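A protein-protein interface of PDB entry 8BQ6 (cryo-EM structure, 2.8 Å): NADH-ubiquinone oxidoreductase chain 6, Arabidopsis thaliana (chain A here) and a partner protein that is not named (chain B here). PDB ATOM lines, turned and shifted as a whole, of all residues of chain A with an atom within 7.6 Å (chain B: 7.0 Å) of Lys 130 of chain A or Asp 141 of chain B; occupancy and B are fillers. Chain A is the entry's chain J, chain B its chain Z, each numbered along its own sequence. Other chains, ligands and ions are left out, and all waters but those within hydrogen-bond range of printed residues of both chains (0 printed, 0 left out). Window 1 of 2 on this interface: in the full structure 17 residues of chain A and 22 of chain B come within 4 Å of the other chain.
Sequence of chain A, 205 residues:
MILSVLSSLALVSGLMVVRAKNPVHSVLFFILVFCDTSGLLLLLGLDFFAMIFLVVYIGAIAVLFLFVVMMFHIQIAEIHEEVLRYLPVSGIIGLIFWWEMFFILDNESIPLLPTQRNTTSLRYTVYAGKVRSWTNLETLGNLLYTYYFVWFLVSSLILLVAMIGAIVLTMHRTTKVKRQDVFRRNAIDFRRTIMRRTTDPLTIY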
ATOM      1  N   ARG A 123     -19.834  19.834  16.887  1.00  0.00           N
ATOM      2  CA  ARG A 123     -18.873  19.514  15.846  1.00  0.00           C
ATOM      3  C   ARG A 123     -19.585  18.777  14.719  1.00  0.00           C
ATOM      4  O   ARG A 123     -20.136  17.692  14.927  1.00  0.00           O
ATOM      5  CB  ARG A 123     -17.740  18.669  16.420  1.00  0.00           C
ATOM      6  CG  ARG A 123     -16.364  19.094  15.957  1.00  0.00           C
ATOM      7  CD  ARG A 123     -15.309  18.909  17.038  1.00  0.00           C
ATOM      8  NE  ARG A 123     -15.385  19.918  18.088  1.00  0.00           N
ATOM      9  CZ  ARG A 123     -14.662  19.892  19.200  1.00  0.00           C
ATOM     10  NH1 ARG A 123     -13.812  18.908  19.447  1.00  0.00           N
ATOM     11  NH2 ARG A 123     -14.789  20.880  20.081  1.00  0.00           N
ATOM     12  N   TYR A 124     -19.596  19.379  13.535  1.00  0.00           N
ATOM     13  CA  TYR A 124     -20.191  18.769  12.355  1.00  0.00           C
ATOM     14  C   TYR A 124     -19.136  17.956  11.619  1.00  0.00           C
ATOM     15  O   TYR A 124     -18.076  18.482  11.270  1.00  0.00           O
ATOM     16  CB  TYR A 124     -20.763  19.838  11.426  1.00  0.00           C
ATOM     17  CG  TYR A 124     -21.553  19.272  10.276  1.00  0.00           C
ATOM     18  CD1 TYR A 124     -22.331  18.139  10.442  1.00  0.00           C
ATOM     19  CD2 TYR A 124     -21.488  19.846   9.017  1.00  0.00           C
ATOM     20  CE1 TYR A 124     -23.043  17.613   9.395  1.00  0.00           C
ATOM     21  CE2 TYR A 124     -22.197  19.326   7.961  1.00  0.00           C
ATOM     22  CZ  TYR A 124     -22.973  18.209   8.156  1.00  0.00           C
ATOM     23  OH  TYR A 124     -23.682  17.683   7.106  1.00  0.00           O
ATOM     24  N   THR A 125     -19.427  16.680  11.381  1.00  0.00           N
ATOM     25  CA  THR A 125     -18.515  15.785  10.682  1.00  0.00           C
ATOM     26  C   THR A 125     -18.956  15.641   9.233  1.00  0.00           C
ATOM     27  O   THR A 125     -20.126  15.352   8.963  1.00  0.00           O
ATOM     28  CB  THR A 125     -18.464  14.409  11.353  1.00  0.00           C
ATOM     29  OG1 THR A 125     -17.836  14.523  12.635  1.00  0.00           O
ATOM     30  CG2 THR A 125     -17.670  13.430  10.505  1.00  0.00           C
ATOM     31  N   VAL A 126     -18.023  15.847   8.307  1.00  0.00           N
ATOM     32  CA  VAL A 126     -18.253  15.630   6.884  1.00  0.00           C
ATOM     33  C   VAL A 126     -17.437  14.413   6.475  1.00  0.00           C
ATOM     34  O   VAL A 126     -16.205  14.481   6.389  1.00  0.00           O
ATOM     35  CB  VAL A 126     -17.876  16.858   6.045  1.00  0.00           C
ATOM     36  CG1 VAL A 126     -18.052  16.560   4.568  1.00  0.00           C
ATOM     37  CG2 VAL A 126     -18.714  18.052   6.453  1.00  0.00           C
ATOM     38  N   TYR A 127     -18.116  13.300   6.209  1.00  0.00           N
ATOM     39  CA  TYR A 127     -17.406  12.059   5.941  1.00  0.00           C
ATOM     40  C   TYR A 127     -16.787  12.011   4.551  1.00  0.00           C
ATOM     41  O   TYR A 127     -15.906  11.178   4.314  1.00  0.00           O
ATOM     42  CB  TYR A 127     -18.339  10.864   6.111  1.00  0.00           C
ATOM     43  CG  TYR A 127     -18.819  10.621   7.512  1.00  0.00           C
ATOM     44  CD1 TYR A 127     -18.032   9.934   8.423  1.00  0.00           C
ATOM     45  CD2 TYR A 127     -20.071  11.052   7.919  1.00  0.00           C
ATOM     46  CE1 TYR A 127     -18.470   9.699   9.704  1.00  0.00           C
ATOM     47  CE2 TYR A 127     -20.518  10.822   9.198  1.00  0.00           C
ATOM     48  CZ  TYR A 127     -19.713  10.146  10.087  1.00  0.00           C
ATOM     49  OH  TYR A 127     -20.156   9.912  11.367  1.00  0.00           O
ATOM     50  N   ALA A 128     -17.221  12.877   3.633  1.00  0.00           N
ATOM     51  CA  ALA A 128     -16.694  12.836   2.272  1.00  0.00           C
ATOM     52  C   ALA A 128     -15.194  13.096   2.250  1.00  0.00           C
ATOM     53  O   ALA A 128     -14.457  12.458   1.489  1.00  0.00           O
ATOM     54  CB  ALA A 128     -17.427  13.848   1.395  1.00  0.00           C
ATOM     55  N   GLY A 129     -14.720  14.022   3.078  1.00  0.00           N
ATOM     56  CA  GLY A 129     -13.294  14.269   3.156  1.00  0.00           C
ATOM     57  C   GLY A 129     -12.472  13.136   3.735  1.00  0.00           C
ATOM     58  O   GLY A 129     -11.250  13.133   3.566  1.00  0.00           O
ATOM     59  N   LYS A 130     -13.104  12.170   4.400  1.00  0.00           N
ATOM     60  CA  LYS A 130     -12.406  11.116   5.125  1.00  0.00           C
ATOM     61  C   LYS A 130     -12.272   9.816   4.347  1.00  0.00           C
ATOM     62  O   LYS A 130     -11.719   8.853   4.885  1.00  0.00           O
ATOM     63  CB  LYS A 130     -13.128  10.826   6.438  1.00  0.00           C
ATOM     64  CG  LYS A 130     -12.874  11.821   7.528  1.00  0.00           C
ATOM     65  CD  LYS A 130     -13.903  11.667   8.621  1.00  0.00           C
ATOM     66  CE  LYS A 130     -13.551  12.539   9.802  1.00  0.00           C
ATOM     67  NZ  LYS A 130     -13.525  13.973   9.412  1.00  0.00           N
ATOM     68  N   VAL A 131     -12.779   9.752   3.115  1.00  0.00           N
ATOM     69  CA  VAL A 131     -12.737   8.501   2.361  1.00  0.00           C
ATOM     70  C   VAL A 131     -11.301   8.125   2.017  1.00  0.00           C
ATOM     71  O   VAL A 131     -10.868   6.989   2.248  1.00  0.00           O
ATOM     72  CB  VAL A 131     -13.604   8.616   1.096  1.00  0.00           C
ATOM     73  CG1 VAL A 131     -13.309   7.471   0.148  1.00  0.00           C
ATOM     74  CG2 VAL A 131     -15.074   8.634   1.462  1.00  0.00           C
ATOM     75  N   ARG A 132     -10.548   9.068   1.449  1.00  0.00           N
ATOM     76  CA  ARG A 132      -9.134   8.892   1.105  1.00  0.00           C
ATOM     77  C   ARG A 132      -8.429  10.156   1.589  1.00  0.00           C
ATOM     78  O   ARG A 132      -8.340  11.146   0.859  1.00  0.00           O
ATOM     79  CB  ARG A 132      -8.931   8.671  -0.391  1.00  0.00           C
ATOM     80  CG  ARG A 132      -7.468   8.528  -0.813  1.00  0.00           C
ATOM     81  CD  ARG A 132      -7.320   8.387  -2.327  1.00  0.00           C
ATOM     82  NE  ARG A 132      -5.924   8.340  -2.747  1.00  0.00           N
ATOM     83  CZ  ARG A 132      -5.523   8.029  -3.973  1.00  0.00           C
ATOM     84  NH1 ARG A 132      -6.388   7.761  -4.937  1.00  0.00           N
ATOM     85  NH2 ARG A 132      -4.219   7.976  -4.235  1.00  0.00           N
ATOM     86  N   SER A 133      -7.941  10.118   2.824  1.00  0.00           N
ATOM     87  CA  SER A 133      -7.256  11.266   3.399  1.00  0.00           C
ATOM     88  C   SER A 133      -5.786  11.281   3.003  1.00  0.00           C
ATOM     89  O   SER A 133      -5.187  10.238   2.728  1.00  0.00           O
ATOM     90  CB  SER A 133      -7.378  11.244   4.914  1.00  0.00           C
ATOM     91  OG  SER A 133      -7.060   9.954   5.416  1.00  0.00           O
ATOM     92  N   TYR B  79     -11.919   1.680  -0.890  1.00  0.00           N
ATOM     93  CA  TYR B  79     -12.490   3.003  -1.148  1.00  0.00           C
ATOM     94  C   TYR B  79     -13.888   2.919  -1.766  1.00  0.00           C
ATOM     95  O   TYR B  79     -14.738   3.774  -1.490  1.00  0.00           O
ATOM     96  CB  TYR B  79     -11.550   3.810  -2.045  1.00  0.00           C
ATOM     97  CG  TYR B  79     -10.230   4.200  -1.399  1.00  0.00           C
ATOM     98  CD1 TYR B  79     -10.080   4.234  -0.020  1.00  0.00           C
ATOM     99  CD2 TYR B  79      -9.125   4.505  -2.179  1.00  0.00           C
ATOM    100  CE1 TYR B  79      -8.871   4.591   0.558  1.00  0.00           C
ATOM    101  CE2 TYR B  79      -7.915   4.850  -1.608  1.00  0.00           C
ATOM    102  CZ  TYR B  79      -7.791   4.889  -0.242  1.00  0.00           C
ATOM    103  OH  TYR B  79      -6.581   5.236   0.313  1.00  0.00           O
ATOM    104  N   ARG B  82     -16.214   2.204   1.121  1.00  0.00           N
ATOM    105  CA  ARG B  82     -16.473   3.419   1.883  1.00  0.00           C
ATOM    106  C   ARG B  82     -17.398   4.379   1.144  1.00  0.00           C
ATOM    107  O   ARG B  82     -18.166   5.107   1.781  1.00  0.00           O
ATOM    108  CB  ARG B  82     -15.160   4.109   2.217  1.00  0.00           C
ATOM    109  CG  ARG B  82     -14.438   3.474   3.365  1.00  0.00           C
ATOM    110  CD  ARG B  82     -13.078   4.077   3.504  1.00  0.00           C
ATOM    111  NE  ARG B  82     -12.306   3.415   4.542  1.00  0.00           N
ATOM    112  CZ  ARG B  82     -11.236   3.944   5.113  1.00  0.00           C
ATOM    113  NH1 ARG B  82     -10.790   5.140   4.766  1.00  0.00           N
ATOM    114  NH2 ARG B  82     -10.606   3.265   6.065  1.00  0.00           N
ATOM    115  N   GLU B 137     -10.462  25.207  18.218  1.00  0.00           N
ATOM    116  CA  GLU B 137      -9.361  24.270  18.374  1.00  0.00           C
ATOM    117  C   GLU B 137      -8.660  24.155  17.034  1.00  0.00           C
ATOM    118  O   GLU B 137      -9.315  23.991  16.001  1.00  0.00           O
ATOM    119  CB  GLU B 137      -9.859  22.909  18.839  1.00  0.00           C
ATOM    120  CG  GLU B 137      -9.794  22.750  20.330  1.00  0.00           C
ATOM    121  CD  GLU B 137     -11.008  22.049  20.865  1.00  0.00           C
ATOM    122  OE1 GLU B 137     -11.948  21.820  20.075  1.00  0.00           O
ATOM    123  OE2 GLU B 137     -11.036  21.747  22.074  1.00  0.00           O
ATOM    124  N   LEU B 138      -7.334  24.252  17.055  1.00  0.00           N
ATOM    125  CA  LEU B 138      -6.587  24.397  15.813  1.00  0.00           C
ATOM    126  C   LEU B 138      -6.728  23.163  14.930  1.00  0.00           C
ATOM    127  O   LEU B 138      -7.158  23.258  13.776  1.00  0.00           O
ATOM    128  CB  LEU B 138      -5.125  24.683  16.136  1.00  0.00           C
ATOM    129  CG  LEU B 138      -4.707  26.095  15.749  1.00  0.00           C
ATOM    130  CD1 LEU B 138      -3.311  26.388  16.218  1.00  0.00           C
ATOM    131  CD2 LEU B 138      -4.775  26.193  14.262  1.00  0.00           C
ATOM    132  N   ARG B 139      -6.397  21.992  15.464  1.00  0.00           N
ATOM    133  CA  ARG B 139      -6.434  20.741  14.707  1.00  0.00           C
ATOM    134  C   ARG B 139      -7.139  19.671  15.531  1.00  0.00           C
ATOM    135  O   ARG B 139      -6.505  18.729  16.022  1.00  0.00           O
ATOM    136  CB  ARG B 139      -5.022  20.299  14.327  1.00  0.00           C
ATOM    137  CG  ARG B 139      -4.957  19.375  13.129  1.00  0.00           C
ATOM    138  CD  ARG B 139      -4.697  20.134  11.847  1.00  0.00           C
ATOM    139  NE  ARG B 139      -4.834  19.286  10.670  1.00  0.00           N
ATOM    140  CZ  ARG B 139      -3.821  18.715  10.035  1.00  0.00           C
ATOM    141  NH1 ARG B 139      -2.576  18.844  10.463  1.00  0.00           N
ATOM    142  NH2 ARG B 139      -4.060  18.004   8.937  1.00  0.00           N
ATOM    143  N   PRO B 140      -8.458  19.784  15.701  1.00  0.00           N
ATOM    144  CA  PRO B 140      -9.172  18.782  16.508  1.00  0.00           C
ATOM    145  C   PRO B 140      -9.416  17.464  15.789  1.00  0.00           C
ATOM    146  O   PRO B 140      -9.722  16.470  16.459  1.00  0.00           O
ATOM    147  CB  PRO B 140     -10.493  19.482  16.851  1.00  0.00           C
ATOM    148  CG  PRO B 140     -10.705  20.452  15.744  1.00  0.00           C
ATOM    149  CD  PRO B 140      -9.350  20.858  15.226  1.00  0.00           C
ATOM    150  N   ASP B 141      -9.299  17.409  14.461  1.00  0.00           N
ATOM    151  CA  ASP B 141      -9.610  16.166  13.763  1.00  0.00           C
ATOM    152  C   ASP B 141      -8.517  15.113  13.905  1.00  0.00           C
ATOM    153  O   ASP B 141      -8.812  13.921  13.781  1.00  0.00           O
ATOM    154  CB  ASP B 141      -9.873  16.428  12.279  1.00  0.00           C
ATOM    155  CG  ASP B 141     -10.954  15.523  11.710  1.00  0.00           C
ATOM    156  OD1 ASP B 141     -10.841  14.287  11.862  1.00  0.00           O
ATOM    157  OD2 ASP B 141     -11.909  16.041  11.096  1.00  0.00           O
ATOM    158  N   VAL B 142      -7.268  15.513  14.172  1.00  0.00           N
ATOM    159  CA  VAL B 142      -6.156  14.567  14.155  1.00  0.00           C
ATOM    160  C   VAL B 142      -5.933  13.868  15.489  1.00  0.00           C
ATOM    161  O   VAL B 142      -5.061  12.993  15.577  1.00  0.00           O
ATOM    162  CB  VAL B 142      -4.841  15.256  13.737  1.00  0.00           C
ATOM    163  CG1 VAL B 142      -4.980  15.877  12.359  1.00  0.00           C
ATOM    164  CG2 VAL B 142      -4.444  16.298  14.769  1.00  0.00           C
ATOM    165  N   TRP B 143      -6.676  14.226  16.529  1.00  0.00           N
ATOM    166  CA  TRP B 143      -6.471  13.608  17.835  1.00  0.00           C
ATOM    167  C   TRP B 143      -7.729  12.901  18.322  1.00  0.00           C
ATOM    168  O   TRP B 143      -8.530  12.421  17.523  1.00  0.00           O
ATOM    169  CB  TRP B 143      -6.034  14.654  18.859  1.00  0.00           C
ATOM    170  CG  TRP B 143      -4.613  15.079  18.714  1.00  0.00           C
ATOM    171  CD1 TRP B 143      -4.166  16.265  18.219  1.00  0.00           C
ATOM    172  CD2 TRP B 143      -3.448  14.329  19.075  1.00  0.00           C
ATOM    173  NE1 TRP B 143      -2.795  16.302  18.243  1.00  0.00           N
ATOM    174  CE2 TRP B 143      -2.329  15.125  18.764  1.00  0.00           C
ATOM    175  CE3 TRP B 143      -3.241  13.062  19.627  1.00  0.00           C
ATOM    176  CZ2 TRP B 143      -1.025  14.699  18.989  1.00  0.00           C
ATOM    177  CZ3 TRP B 143      -1.945  12.641  19.849  1.00  0.00           C
ATOM    178  CH2 TRP B 143      -0.854  13.457  19.531  1.00  0.00           C
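Of the 11 printed residues of chain A, 4 touch a printed residue of chain B. Among the printed residues, Asp or Glu carboxylates within 4 Å of a Lys or Arg side-chain nitrogen of the other chain: Arg 123 of chain A with Glu 137 of chain B and Lys 130 of chain A with Asp 141 of chain B.
Lys 130 of chain A touches just these residues of chain B: Arg 82 and Asp 141. Of chain A, only Lys 130 (3.1 Å) comes within 4 Å of Asp 141 of chain B. No residue of chain B comes within 4 Å of Gly 129 of chain A. Of the printed residues of chain A, Glu 137 of chain B touches Arg 123. Of the printed residues of chain A, Arg 82 of chain B touches Lys 130 and Val 131. Printed residues of chain B within 4 Å of Val 131 of chain A: Tyr 79 and Arg 82. Of the printed residues of chain A, Tyr 79 of chain B touches Val 131 and Arg 132. Ser 133 of chain A touches none of the printed residues of chain B. The nearest residue of chain A that does not touch Asp 141 of chain B is Thr 125 of chain A (6.3 Å). The nearest printed residue of chain A that does not touch Arg 82 of chain B is Arg 132 of chain A (5.1 Å).
Among the printed residues, merely in contact across the chains: Val 131 of chain A with Tyr 79 of chain B, Arg 132 of chain A with Tyr 79 of chain B and Lys 130 of chain A with Arg 82 of chain B.
OE1 of Glu 137 of chain B lies within salt-bridge range of NH2 of Arg 123 of chain A. NZ of Lys 130 of chain A is in salt-bridge range of OD2 of Asp 141 of chain B (3.1 Å). NH1 of Arg 82 of chain B lies within hydrogen-bond range of O of Val 131 of chain A, at 3.1 Å.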
